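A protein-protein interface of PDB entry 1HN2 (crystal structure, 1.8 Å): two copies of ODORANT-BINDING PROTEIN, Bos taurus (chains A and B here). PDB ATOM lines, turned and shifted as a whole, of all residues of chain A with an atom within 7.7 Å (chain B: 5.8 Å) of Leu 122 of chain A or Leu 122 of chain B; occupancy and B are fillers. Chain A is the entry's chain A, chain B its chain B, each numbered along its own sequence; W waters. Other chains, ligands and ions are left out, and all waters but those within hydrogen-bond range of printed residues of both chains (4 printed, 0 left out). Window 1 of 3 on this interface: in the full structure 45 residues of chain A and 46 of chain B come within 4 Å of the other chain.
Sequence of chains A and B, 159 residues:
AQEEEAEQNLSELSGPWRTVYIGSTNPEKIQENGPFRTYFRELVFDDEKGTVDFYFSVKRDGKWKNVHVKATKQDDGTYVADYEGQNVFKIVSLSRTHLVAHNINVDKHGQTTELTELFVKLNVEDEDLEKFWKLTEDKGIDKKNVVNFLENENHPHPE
Water W2 lies within hydrogen-bond range of the side-chain carboxylate (OE2) of Glu 153 of chain B, the guanidinium group (NE) of Arg 18 of chain A and the guanidinium group (NE) of Arg 18 of chain B.
Water W3 lies within hydrogen-bond range of OE1 of Glu 153 of chain B (2.7 Å), O of Phe 40 of chain A (3.0 Å) and N of Thr 19 of chain A (3.1 Å).
Water W4 bridges O of Lys 121 of chain A (2.9 Å) and N of Asn 123 of chain B (3.1 Å).
Water W1 lies within hydrogen-bond range of OE1 of Glu 153 of chain B and O of Phe 40 of chain A.
Leu 13 of chain A touches none of the printed residues of chain B.
Printed residues of chain B within 4 Å of Val 20 of chain A: Leu 150 (3.5 Å).
Of chain B, only Leu 122 (3.8 Å) comes within 4 Å of Leu 122 of chain A.
Printed residues of chain B within 4 Å of Asn 123 of chain A: Val 120 (3.4 Å).
Of the printed residues of chain A, Val 120 of chain B touches Asn 123.
Printed residues of chain A within 4 Å of Leu 122 of chain B: Leu 122 (3.8 Å).
The nearest printed residue of chain B that does not touch Asn 123 of chain A is Lys 121 of chain B (5.9 Å).
The backbone carbonyl oxygen of Arg 96 of chain A lies within hydrogen-bond range of the side-chain amide nitrogen of Asn 123 of chain A (3.2 Å).
The backbone NH of Leu 122 of chain A sits at hydrogen-bond distance from the backbone carbonyl oxygen of Pro 16 of chain A (2.9 Å).
The backbone NH (N) of Leu 122 of chain B is in hydrogen-bond range of the backbone carbonyl oxygen (O) of Pro 16 of chain B, 3.0 Å away.
N of Phe 40 of chain A lies within hydrogen-bond range of OG1 of Thr 19 of chain A.
The backbone NH (N) of Arg 18 of chain B lies within hydrogen-bond range of the backbone carbonyl oxygen (O) of Val 120 of chain B, at 2.7 Å.
Of the 20 printed residues of chain A, 4 touch a printed residue of chain B.
Hydrophobic or aromatic side chains of chain A that line the printed part of chain B: Leu 122.
Of the 10 printed residues of chain B, 3 touch a printed residue of chain A.
Hydrophobic or aromatic side chains of chain B within 4 Å of the printed part of chain A: Val 120 and Leu 122.
Among the printed residues, 4 pairs touch across the chains.
Leu 122 of chain B touches its own counterpart, Leu 122 of chain A.
Asn 123 of chain A touches Val 120 of chain B, but with the chains exchanged Val 120 of chain A does not touch Asn 123 of chain B (4.02 Å).
Of the 4 pairs that touch across the chains among the printed residues, 1 has its exchanged pair printed and touching as well.
Leu 150 of chain B touches Thr 19 of chain A.
O of Val 20 of chain A touches N of Leu 150 of chain B, at 3.5 Å.
Leu 122 of chain A touches Leu 122 of chain B.
Val 120 of chain B touches Asn 123 of chain A (CG2 to O, 3.4 Å).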
ATOM      1  N   LEU A  13      11.638  16.359 -22.252  1.00  0.00           N
ATOM      2  CA  LEU A  13      12.985  16.916 -22.296  1.00  0.00           C
ATOM      3  C   LEU A  13      13.209  18.250 -21.597  1.00  0.00           C
ATOM      4  O   LEU A  13      14.346  18.723 -21.515  1.00  0.00           O
ATOM      5  CB  LEU A  13      13.438  17.021 -23.752  1.00  0.00           C
ATOM      6  CG  LEU A  13      13.530  15.691 -24.510  1.00  0.00           C
ATOM      7  CD1 LEU A  13      12.150  15.076 -24.669  1.00  0.00           C
ATOM      8  CD2 LEU A  13      14.142  15.933 -25.875  1.00  0.00           C
ATOM      9  N   SER A  14      12.140  18.854 -21.088  1.00  0.00           N
ATOM     10  CA  SER A  14      12.257  20.139 -20.403  1.00  0.00           C
ATOM     11  C   SER A  14      13.160  20.019 -19.179  1.00  0.00           C
ATOM     12  O   SER A  14      13.182  18.986 -18.512  1.00  0.00           O
ATOM     13  CB  SER A  14      10.877  20.638 -19.969  1.00  0.00           C
ATOM     14  OG  SER A  14      10.020  20.801 -21.085  1.00  0.00           O
ATOM     15  N   GLY A  15      13.903  21.079 -18.892  1.00  0.00           N
ATOM     16  CA  GLY A  15      14.787  21.066 -17.746  1.00  0.00           C
ATOM     17  C   GLY A  15      16.053  21.858 -17.986  1.00  0.00           C
ATOM     18  O   GLY A  15      16.137  22.636 -18.934  1.00  0.00           O
ATOM     19  N   PRO A  16      17.062  21.691 -17.125  1.00  0.00           N
ATOM     20  CA  PRO A  16      18.318  22.422 -17.293  1.00  0.00           C
ATOM     21  C   PRO A  16      19.186  21.858 -18.418  1.00  0.00           C
ATOM     22  O   PRO A  16      19.454  20.662 -18.473  1.00  0.00           O
ATOM     23  CB  PRO A  16      18.975  22.295 -15.917  1.00  0.00           C
ATOM     24  CG  PRO A  16      18.479  20.971 -15.426  1.00  0.00           C
ATOM     25  CD  PRO A  16      17.026  20.971 -15.838  1.00  0.00           C
ATOM     26  N   TRP A  17      19.611  22.738 -19.318  1.00  0.00           N
ATOM     27  CA  TRP A  17      20.463  22.365 -20.442  1.00  0.00           C
ATOM     28  C   TRP A  17      21.665  23.294 -20.461  1.00  0.00           C
ATOM     29  O   TRP A  17      21.607  24.417 -19.945  1.00  0.00           O
ATOM     30  CB  TRP A  17      19.720  22.508 -21.777  1.00  0.00           C
ATOM     31  CG  TRP A  17      18.685  21.464 -22.028  1.00  0.00           C
ATOM     32  CD1 TRP A  17      17.461  21.353 -21.433  1.00  0.00           C
ATOM     33  CD2 TRP A  17      18.785  20.377 -22.950  1.00  0.00           C
ATOM     34  NE1 TRP A  17      16.791  20.260 -21.930  1.00  0.00           N
ATOM     35  CE2 TRP A  17      17.581  19.643 -22.862  1.00  0.00           C
ATOM     36  CE3 TRP A  17      19.779  19.947 -23.837  1.00  0.00           C
ATOM     37  CZ2 TRP A  17      17.340  18.503 -23.637  1.00  0.00           C
ATOM     38  CZ3 TRP A  17      19.544  18.813 -24.606  1.00  0.00           C
ATOM     39  CH2 TRP A  17      18.333  18.105 -24.499  1.00  0.00           C
ATOM     40  N   ARG A  18      22.748  22.827 -21.067  1.00  0.00           N
ATOM     41  CA  ARG A  18      23.963  23.621 -21.162  1.00  0.00           C
ATOM     42  C   ARG A  18      24.541  23.576 -22.574  1.00  0.00           C
ATOM     43  O   ARG A  18      24.399  22.587 -23.295  1.00  0.00           O
ATOM     44  CB  ARG A  18      25.018  23.106 -20.172  1.00  0.00           C
ATOM     45  CG  ARG A  18      24.623  23.186 -18.710  1.00  0.00           C
ATOM     46  CD  ARG A  18      24.618  24.629 -18.194  1.00  0.00           C
ATOM     47  NE  ARG A  18      24.295  24.702 -16.767  1.00  0.00           N
ATOM     48  CZ  ARG A  18      23.062  24.703 -16.262  1.00  0.00           C
ATOM     49  NH1 ARG A  18      22.004  24.638 -17.059  1.00  0.00           N
ATOM     50  NH2 ARG A  18      22.886  24.778 -14.947  1.00  0.00           N
ATOM     51  N   THR A  19      25.202  24.662 -22.956  1.00  0.00           N
ATOM     52  CA  THR A  19      25.836  24.767 -24.263  1.00  0.00           C
ATOM     53  C   THR A  19      27.177  24.038 -24.238  1.00  0.00           C
ATOM     54  O   THR A  19      27.965  24.221 -23.300  1.00  0.00           O
ATOM     55  CB  THR A  19      26.127  26.235 -24.612  1.00  0.00           C
ATOM     56  OG1 THR A  19      24.927  27.002 -24.469  1.00  0.00           O
ATOM     57  CG2 THR A  19      26.650  26.355 -26.053  1.00  0.00           C
ATOM     58  N   VAL A  20      27.430  23.212 -25.253  1.00  0.00           N
ATOM     59  CA  VAL A  20      28.711  22.507 -25.347  1.00  0.00           C
ATOM     60  C   VAL A  20      29.508  23.211 -26.445  1.00  0.00           C
ATOM     61  O   VAL A  20      30.584  23.737 -26.189  1.00  0.00           O
ATOM     62  CB  VAL A  20      28.545  21.012 -25.717  1.00  0.00           C
ATOM     63  CG1 VAL A  20      29.914  20.333 -25.739  1.00  0.00           C
ATOM     64  CG2 VAL A  20      27.641  20.311 -24.698  1.00  0.00           C
ATOM     65  N   PHE A  40      23.427  28.410 -22.435  1.00  0.00           N
ATOM     66  CA  PHE A  40      22.098  27.927 -22.081  1.00  0.00           C
ATOM     67  C   PHE A  40      21.961  27.610 -20.601  1.00  0.00           C
ATOM     68  O   PHE A  40      22.930  27.233 -19.935  1.00  0.00           O
ATOM     69  CB  PHE A  40      21.760  26.685 -22.913  1.00  0.00           C
ATOM     70  CG  PHE A  40      21.190  27.001 -24.274  1.00  0.00           C
ATOM     71  CD1 PHE A  40      21.582  28.148 -24.962  1.00  0.00           C
ATOM     72  CD2 PHE A  40      20.276  26.133 -24.877  1.00  0.00           C
ATOM     73  CE1 PHE A  40      21.074  28.426 -26.232  1.00  0.00           C
ATOM     74  CE2 PHE A  40      19.764  26.404 -26.147  1.00  0.00           C
ATOM     75  CZ  PHE A  40      20.163  27.551 -26.824  1.00  0.00           C
ATOM     76  N   ARG A  41      20.747  27.784 -20.089  1.00  0.00           N
ATOM     77  CA  ARG A  41      20.456  27.503 -18.692  1.00  0.00           C
ATOM     78  C   ARG A  41      19.280  26.537 -18.599  1.00  0.00           C
ATOM     79  O   ARG A  41      19.336  25.539 -17.882  1.00  0.00           O
ATOM     80  CB  ARG A  41      20.097  28.785 -17.934  1.00  0.00           C
ATOM     81  CG  ARG A  41      21.190  29.830 -17.840  1.00  0.00           C
ATOM     82  CD  ARG A  41      20.848  30.851 -16.755  1.00  0.00           C
ATOM     83  NE  ARG A  41      19.502  31.405 -16.907  1.00  0.00           N
ATOM     84  CZ  ARG A  41      19.198  32.443 -17.679  1.00  0.00           C
ATOM     85  NH1 ARG A  41      17.945  32.871 -17.757  1.00  0.00           N
ATOM     86  NH2 ARG A  41      20.148  33.066 -18.360  1.00  0.00           N
ATOM     87  N   ARG A  96      17.264  12.124 -24.891  1.00  0.00           N
ATOM     88  CA  ARG A  96      17.083  12.493 -23.494  1.00  0.00           C
ATOM     89  C   ARG A  96      18.288  13.229 -22.914  1.00  0.00           C
ATOM     90  O   ARG A  96      18.199  13.823 -21.840  1.00  0.00           O
ATOM     91  CB  ARG A  96      16.812  11.242 -22.653  1.00  0.00           C
ATOM     92  CG  ARG A  96      15.521  10.535 -22.969  1.00  0.00           C
ATOM     93  CD  ARG A  96      15.392   9.263 -22.160  1.00  0.00           C
ATOM     94  NE  ARG A  96      14.086   8.628 -22.319  1.00  0.00           N
ATOM     95  CZ  ARG A  96      12.939   9.162 -21.910  1.00  0.00           C
ATOM     96  NH1 ARG A  96      12.930  10.347 -21.314  1.00  0.00           N
ATOM     97  NH2 ARG A  96      11.800   8.509 -22.094  1.00  0.00           N
ATOM     98  N   THR A  97      19.410  13.199 -23.625  1.00  0.00           N
ATOM     99  CA  THR A  97      20.624  13.837 -23.132  1.00  0.00           C
ATOM    100  C   THR A  97      21.265  14.894 -24.029  1.00  0.00           C
ATOM    101  O   THR A  97      22.060  15.705 -23.548  1.00  0.00           O
ATOM    102  CB  THR A  97      21.706  12.785 -22.839  1.00  0.00           C
ATOM    103  OG1 THR A  97      22.075  12.132 -24.061  1.00  0.00           O
ATOM    104  CG2 THR A  97      21.188  11.748 -21.860  1.00  0.00           C
ATOM    105  N   PHE A 119      24.021  20.885 -27.471  1.00  0.00           N
ATOM    106  CA  PHE A 119      23.642  21.200 -26.097  1.00  0.00           C
ATOM    107  C   PHE A 119      23.406  19.888 -25.370  1.00  0.00           C
ATOM    108  O   PHE A 119      22.972  18.911 -25.976  1.00  0.00           O
ATOM    109  CB  PHE A 119      22.368  22.048 -26.070  1.00  0.00           C
ATOM    110  CG  PHE A 119      22.433  23.253 -26.962  1.00  0.00           C
ATOM    111  CD1 PHE A 119      22.094  23.156 -28.309  1.00  0.00           C
ATOM    112  CD2 PHE A 119      22.872  24.478 -26.464  1.00  0.00           C
ATOM    113  CE1 PHE A 119      22.196  24.268 -29.155  1.00  0.00           C
ATOM    114  CE2 PHE A 119      22.981  25.596 -27.296  1.00  0.00           C
ATOM    115  CZ  PHE A 119      22.644  25.493 -28.644  1.00  0.00           C
ATOM    116  N   VAL A 120      23.713  19.862 -24.077  1.00  0.00           N
ATOM    117  CA  VAL A 120      23.525  18.657 -23.286  1.00  0.00           C
ATOM    118  C   VAL A 120      22.624  18.951 -22.101  1.00  0.00           C
ATOM    119  O   VAL A 120      22.642  20.050 -21.544  1.00  0.00           O
ATOM    120  CB  VAL A 120      24.876  18.090 -22.777  1.00  0.00           C
ATOM    121  CG1 VAL A 120      25.737  17.693 -23.955  1.00  0.00           C
ATOM    122  CG2 VAL A 120      25.593  19.118 -21.909  1.00  0.00           C
ATOM    123  N   LYS A 121      21.825  17.963 -21.723  1.00  0.00           N
ATOM    124  CA  LYS A 121      20.907  18.134 -20.615  1.00  0.00           C
ATOM    125  C   LYS A 121      21.489  17.644 -19.300  1.00  0.00           C
ATOM    126  O   LYS A 121      22.210  16.648 -19.255  1.00  0.00           O
ATOM    127  CB  LYS A 121      19.593  17.395 -20.889  1.00  0.00           C
ATOM    128  CG  LYS A 121      18.559  17.612 -19.807  1.00  0.00           C
ATOM    129  CD  LYS A 121      17.274  16.858 -20.038  1.00  0.00           C
ATOM    130  CE  LYS A 121      16.293  17.137 -18.893  1.00  0.00           C
ATOM    131  NZ  LYS A 121      14.978  16.461 -19.056  1.00  0.00           N
ATOM    132  N   LEU A 122      21.193  18.367 -18.230  1.00  0.00           N
ATOM    133  CA  LEU A 122      21.654  17.964 -16.909  1.00  0.00           C
ATOM    134  C   LEU A 122      20.497  17.194 -16.306  1.00  0.00           C
ATOM    135  O   LEU A 122      19.538  17.783 -15.824  1.00  0.00           O
ATOM    136  CB  LEU A 122      21.982  19.177 -16.048  1.00  0.00           C
ATOM    137  CG  LEU A 122      23.320  19.836 -16.369  1.00  0.00           C
ATOM    138  CD1 LEU A 122      23.332  20.302 -17.814  1.00  0.00           C
ATOM    139  CD2 LEU A 122      23.549  20.997 -15.422  1.00  0.00           C
ATOM    140  N   ASN A 123      20.592  15.873 -16.354  1.00  0.00           N
ATOM    141  CA  ASN A 123      19.535  15.013 -15.842  1.00  0.00           C
ATOM    142  C   ASN A 123      19.692  14.651 -14.373  1.00  0.00           C
ATOM    143  O   ASN A 123      20.713  14.110 -13.973  1.00  0.00           O
ATOM    144  CB  ASN A 123      19.466  13.729 -16.673  1.00  0.00           C
ATOM    145  CG  ASN A 123      19.006  13.982 -18.092  1.00  0.00           C
ATOM    146  OD1 ASN A 123      17.909  14.499 -18.313  1.00  0.00           O
ATOM    147  ND2 ASN A 123      19.838  13.620 -19.065  1.00  0.00           N
ATOM    148  N   VAL A 124      18.672  14.958 -13.578  1.00  0.00           N
ATOM    149  CA  VAL A 124      18.682  14.635 -12.158  1.00  0.00           C
ATOM    150  C   VAL A 124      17.619  13.557 -11.955  1.00  0.00           C
ATOM    151  O   VAL A 124      16.419  13.823 -12.067  1.00  0.00           O
ATOM    152  CB  VAL A 124      18.329  15.861 -11.291  1.00  0.00           C
ATOM    153  CG1 VAL A 124      18.412  15.489  -9.822  1.00  0.00           C
ATOM    154  CG2 VAL A 124      19.269  17.017 -11.606  1.00  0.00           C
ATOM    155  N   GLU A 125      18.065  12.339 -11.669  1.00  0.00           N
ATOM    156  CA  GLU A 125      17.157  11.210 -11.476  1.00  0.00           C
ATOM    157  C   GLU A 125      16.458  11.198 -10.120  1.00  0.00           C
ATOM    158  O   GLU A 125      17.030  11.621  -9.114  1.00  0.00           O
ATOM    159  CB  GLU A 125      17.917   9.896 -11.648  1.00  0.00           C
ATOM    160  CG  GLU A 125      18.367   9.617 -13.028  1.00  0.00           C
ATOM    161  CD  GLU A 125      18.971   8.241 -13.146  1.00  0.00           C
ATOM    162  OE1 GLU A 125      18.314   7.277 -12.709  1.00  0.00           O
ATOM    163  OE2 GLU A 125      20.096   8.118 -13.670  1.00  0.00           O
ATOM    164  N   LEU A 150      21.314  24.719  -9.066  1.00  0.00           N
ATOM    165  CA  LEU A 150      20.912  24.642 -10.467  1.00  0.00           C
ATOM    166  C   LEU A 150      20.140  25.889 -10.879  1.00  0.00           C
ATOM    167  O   LEU A 150      20.327  26.416 -11.979  1.00  0.00           O
ATOM    168  CB  LEU A 150      20.066  23.390 -10.693  1.00  0.00           C
ATOM    169  CG  LEU A 150      20.618  22.351 -11.672  1.00  0.00           C
ATOM    170  CD1 LEU A 150      22.104  22.115 -11.443  1.00  0.00           C
ATOM    171  CD2 LEU A 150      19.834  21.062 -11.509  1.00  0.00           C
ATOM    172  N   PRO B  16      33.566  16.941 -16.411  1.00  0.00           N
ATOM    173  CA  PRO B  16      32.757  18.037 -15.862  1.00  0.00           C
ATOM    174  C   PRO B  16      31.628  17.542 -14.966  1.00  0.00           C
ATOM    175  O   PRO B  16      30.875  16.643 -15.333  1.00  0.00           O
ATOM    176  CB  PRO B  16      32.240  18.747 -17.111  1.00  0.00           C
ATOM    177  CG  PRO B  16      32.134  17.634 -18.111  1.00  0.00           C
ATOM    178  CD  PRO B  16      33.406  16.846 -17.873  1.00  0.00           C
ATOM    179  N   TRP B  17      31.538  18.126 -13.781  1.00  0.00           N
ATOM    180  CA  TRP B  17      30.503  17.786 -12.813  1.00  0.00           C
ATOM    181  C   TRP B  17      29.906  19.099 -12.314  1.00  0.00           C
ATOM    182  O   TRP B  17      30.584  20.134 -12.301  1.00  0.00           O
ATOM    183  CB  TRP B  17      31.091  17.015 -11.627  1.00  0.00           C
ATOM    184  CG  TRP B  17      31.395  15.565 -11.893  1.00  0.00           C
ATOM    185  CD1 TRP B  17      32.469  15.063 -12.554  1.00  0.00           C
ATOM    186  CD2 TRP B  17      30.608  14.435 -11.482  1.00  0.00           C
ATOM    187  NE1 TRP B  17      32.413  13.684 -12.581  1.00  0.00           N
ATOM    188  CE2 TRP B  17      31.278  13.273 -11.932  1.00  0.00           C
ATOM    189  CE3 TRP B  17      29.401  14.294 -10.777  1.00  0.00           C
ATOM    190  CZ2 TRP B  17      30.781  11.979 -11.703  1.00  0.00           C
ATOM    191  CZ3 TRP B  17      28.901  13.007 -10.546  1.00  0.00           C
ATOM    192  CH2 TRP B  17      29.596  11.865 -11.010  1.00  0.00           C
ATOM    193  N   ARG B  18      28.645  19.053 -11.896  1.00  0.00           N
ATOM    194  CA  ARG B  18      27.960  20.247 -11.409  1.00  0.00           C
ATOM    195  C   ARG B  18      27.254  19.988 -10.084  1.00  0.00           C
ATOM    196  O   ARG B  18      26.764  18.890  -9.825  1.00  0.00           O
ATOM    197  CB  ARG B  18      26.935  20.718 -12.446  1.00  0.00           C
ATOM    198  CG  ARG B  18      27.531  21.133 -13.760  1.00  0.00           C
ATOM    199  CD  ARG B  18      28.292  22.441 -13.655  1.00  0.00           C
ATOM    200  NE  ARG B  18      28.814  22.870 -14.955  1.00  0.00           N
ATOM    201  CZ  ARG B  18      30.008  22.544 -15.447  1.00  0.00           C
ATOM    202  NH1 ARG B  18      30.370  22.991 -16.644  1.00  0.00           N
ATOM    203  NH2 ARG B  18      30.845  21.790 -14.747  1.00  0.00           N
ATOM    204  N   VAL B 120      25.991  16.123 -10.228  1.00  0.00           N
ATOM    205  CA  VAL B 120      25.651  15.422 -11.450  1.00  0.00           C
ATOM    206  C   VAL B 120      26.744  15.664 -12.482  1.00  0.00           C
ATOM    207  O   VAL B 120      27.338  16.745 -12.543  1.00  0.00           O
ATOM    208  CB  VAL B 120      24.275  15.906 -11.989  1.00  0.00           C
ATOM    209  CG1 VAL B 120      24.319  17.399 -12.268  1.00  0.00           C
ATOM    210  CG2 VAL B 120      23.899  15.147 -13.256  1.00  0.00           C
ATOM    211  N   LYS B 121      27.022  14.642 -13.279  1.00  0.00           N
ATOM    212  CA  LYS B 121      28.040  14.747 -14.304  1.00  0.00           C
ATOM    213  C   LYS B 121      27.446  15.156 -15.644  1.00  0.00           C
ATOM    214  O   LYS B 121      26.339  14.749 -15.997  1.00  0.00           O
ATOM    215  CB  LYS B 121      28.772  13.411 -14.470  1.00  0.00           C
ATOM    216  CG  LYS B 121      29.859  13.478 -15.541  1.00  0.00           C
ATOM    217  CD  LYS B 121      30.524  12.175 -15.795  1.00  0.00           C
ATOM    218  CE  LYS B 121      31.590  12.336 -16.884  1.00  0.00           C
ATOM    219  NZ  LYS B 121      32.217  11.042 -17.220  1.00  0.00           N
ATOM    220  N   LEU B 122      28.186  15.976 -16.382  1.00  0.00           N
ATOM    221  CA  LEU B 122      27.760  16.410 -17.705  1.00  0.00           C
ATOM    222  C   LEU B 122      28.411  15.446 -18.676  1.00  0.00           C
ATOM    223  O   LEU B 122      29.628  15.470 -18.849  1.00  0.00           O
ATOM    224  CB  LEU B 122      28.239  17.832 -17.999  1.00  0.00           C
ATOM    225  CG  LEU B 122      27.292  18.966 -17.614  1.00  0.00           C
ATOM    226  CD1 LEU B 122      26.951  18.870 -16.136  1.00  0.00           C
ATOM    227  CD2 LEU B 122      27.937  20.306 -17.942  1.00  0.00           C
ATOM    228  N   ASN B 123      27.603  14.597 -19.299  1.00  0.00           N
ATOM    229  CA  ASN B 123      28.114  13.606 -20.233  1.00  0.00           C
ATOM    230  C   ASN B 123      27.931  13.971 -21.695  1.00  0.00           C
ATOM    231  O   ASN B 123      26.825  14.276 -22.135  1.00  0.00           O
ATOM    232  CB  ASN B 123      27.453  12.249 -19.978  1.00  0.00           C
ATOM    233  CG  ASN B 123      28.301  11.343 -19.112  1.00  0.00           C
ATOM    234  OD1 ASN B 123      29.416  10.974 -19.485  1.00  0.00           O
ATOM    235  ND2 ASN B 123      27.779  10.980 -17.949  1.00  0.00           N
ATOM    236  N   VAL B 124      29.030  13.941 -22.437  1.00  0.00           N
ATOM    237  CA  VAL B 124      29.011  14.228 -23.864  1.00  0.00           C
ATOM    238  C   VAL B 124      29.434  12.944 -24.574  1.00  0.00           C
ATOM    239  O   VAL B 124      30.586  12.531 -24.479  1.00  0.00           O
ATOM    240  CB  VAL B 124      29.995  15.358 -24.227  1.00  0.00           C
ATOM    241  CG1 VAL B 124      30.027  15.555 -25.737  1.00  0.00           C
ATOM    242  CG2 VAL B 124      29.580  16.648 -23.538  1.00  0.00           C
ATOM    243  N   LEU B 150      31.707  24.625 -22.946  1.00  0.00           N
ATOM    244  CA  LEU B 150      31.888  23.763 -21.793  1.00  0.00           C
ATOM    245  C   LEU B 150      33.209  23.998 -21.075  1.00  0.00           C
ATOM    246  O   LEU B 150      33.252  24.039 -19.843  1.00  0.00           O
ATOM    247  CB  LEU B 150      31.773  22.300 -22.212  1.00  0.00           C
ATOM    248  CG  LEU B 150      31.967  21.269 -21.103  1.00  0.00           C
ATOM    249  CD1 LEU B 150      30.952  21.496 -19.995  1.00  0.00           C
ATOM    250  CD2 LEU B 150      31.821  19.869 -21.695  1.00  0.00           C
ATOM    251  N   GLU B 153      33.086  27.268 -19.132  1.00  0.00           N
ATOM    252  CA  GLU B 153      32.409  27.132 -17.850  1.00  0.00           C
ATOM    253  C   GLU B 153      33.267  26.350 -16.858  1.00  0.00           C
ATOM    254  O   GLU B 153      33.183  26.585 -15.659  1.00  0.00           O
ATOM    255  CB  GLU B 153      31.056  26.429 -18.010  1.00  0.00           C
ATOM    256  CG  GLU B 153      29.990  27.257 -18.665  1.00  0.00           C
ATOM    257  CD  GLU B 153      28.609  26.662 -18.458  1.00  0.00           C
ATOM    258  OE1 GLU B 153      27.628  27.203 -19.000  1.00  0.00           O
ATOM    259  OE2 GLU B 153      28.506  25.644 -17.745  1.00  0.00           O
HETATM  260  O   HOH W   1      25.066  27.968 -17.778  1.00  0.00           O
HETATM  261  O   HOH W   2      26.966  25.055 -15.786  1.00  0.00           O
HETATM  262  O   HOH W   3      25.702  26.890 -20.929  1.00  0.00           O
HETATM  263  O   HOH W   4      24.472  14.878 -19.387  1.00  0.00           O
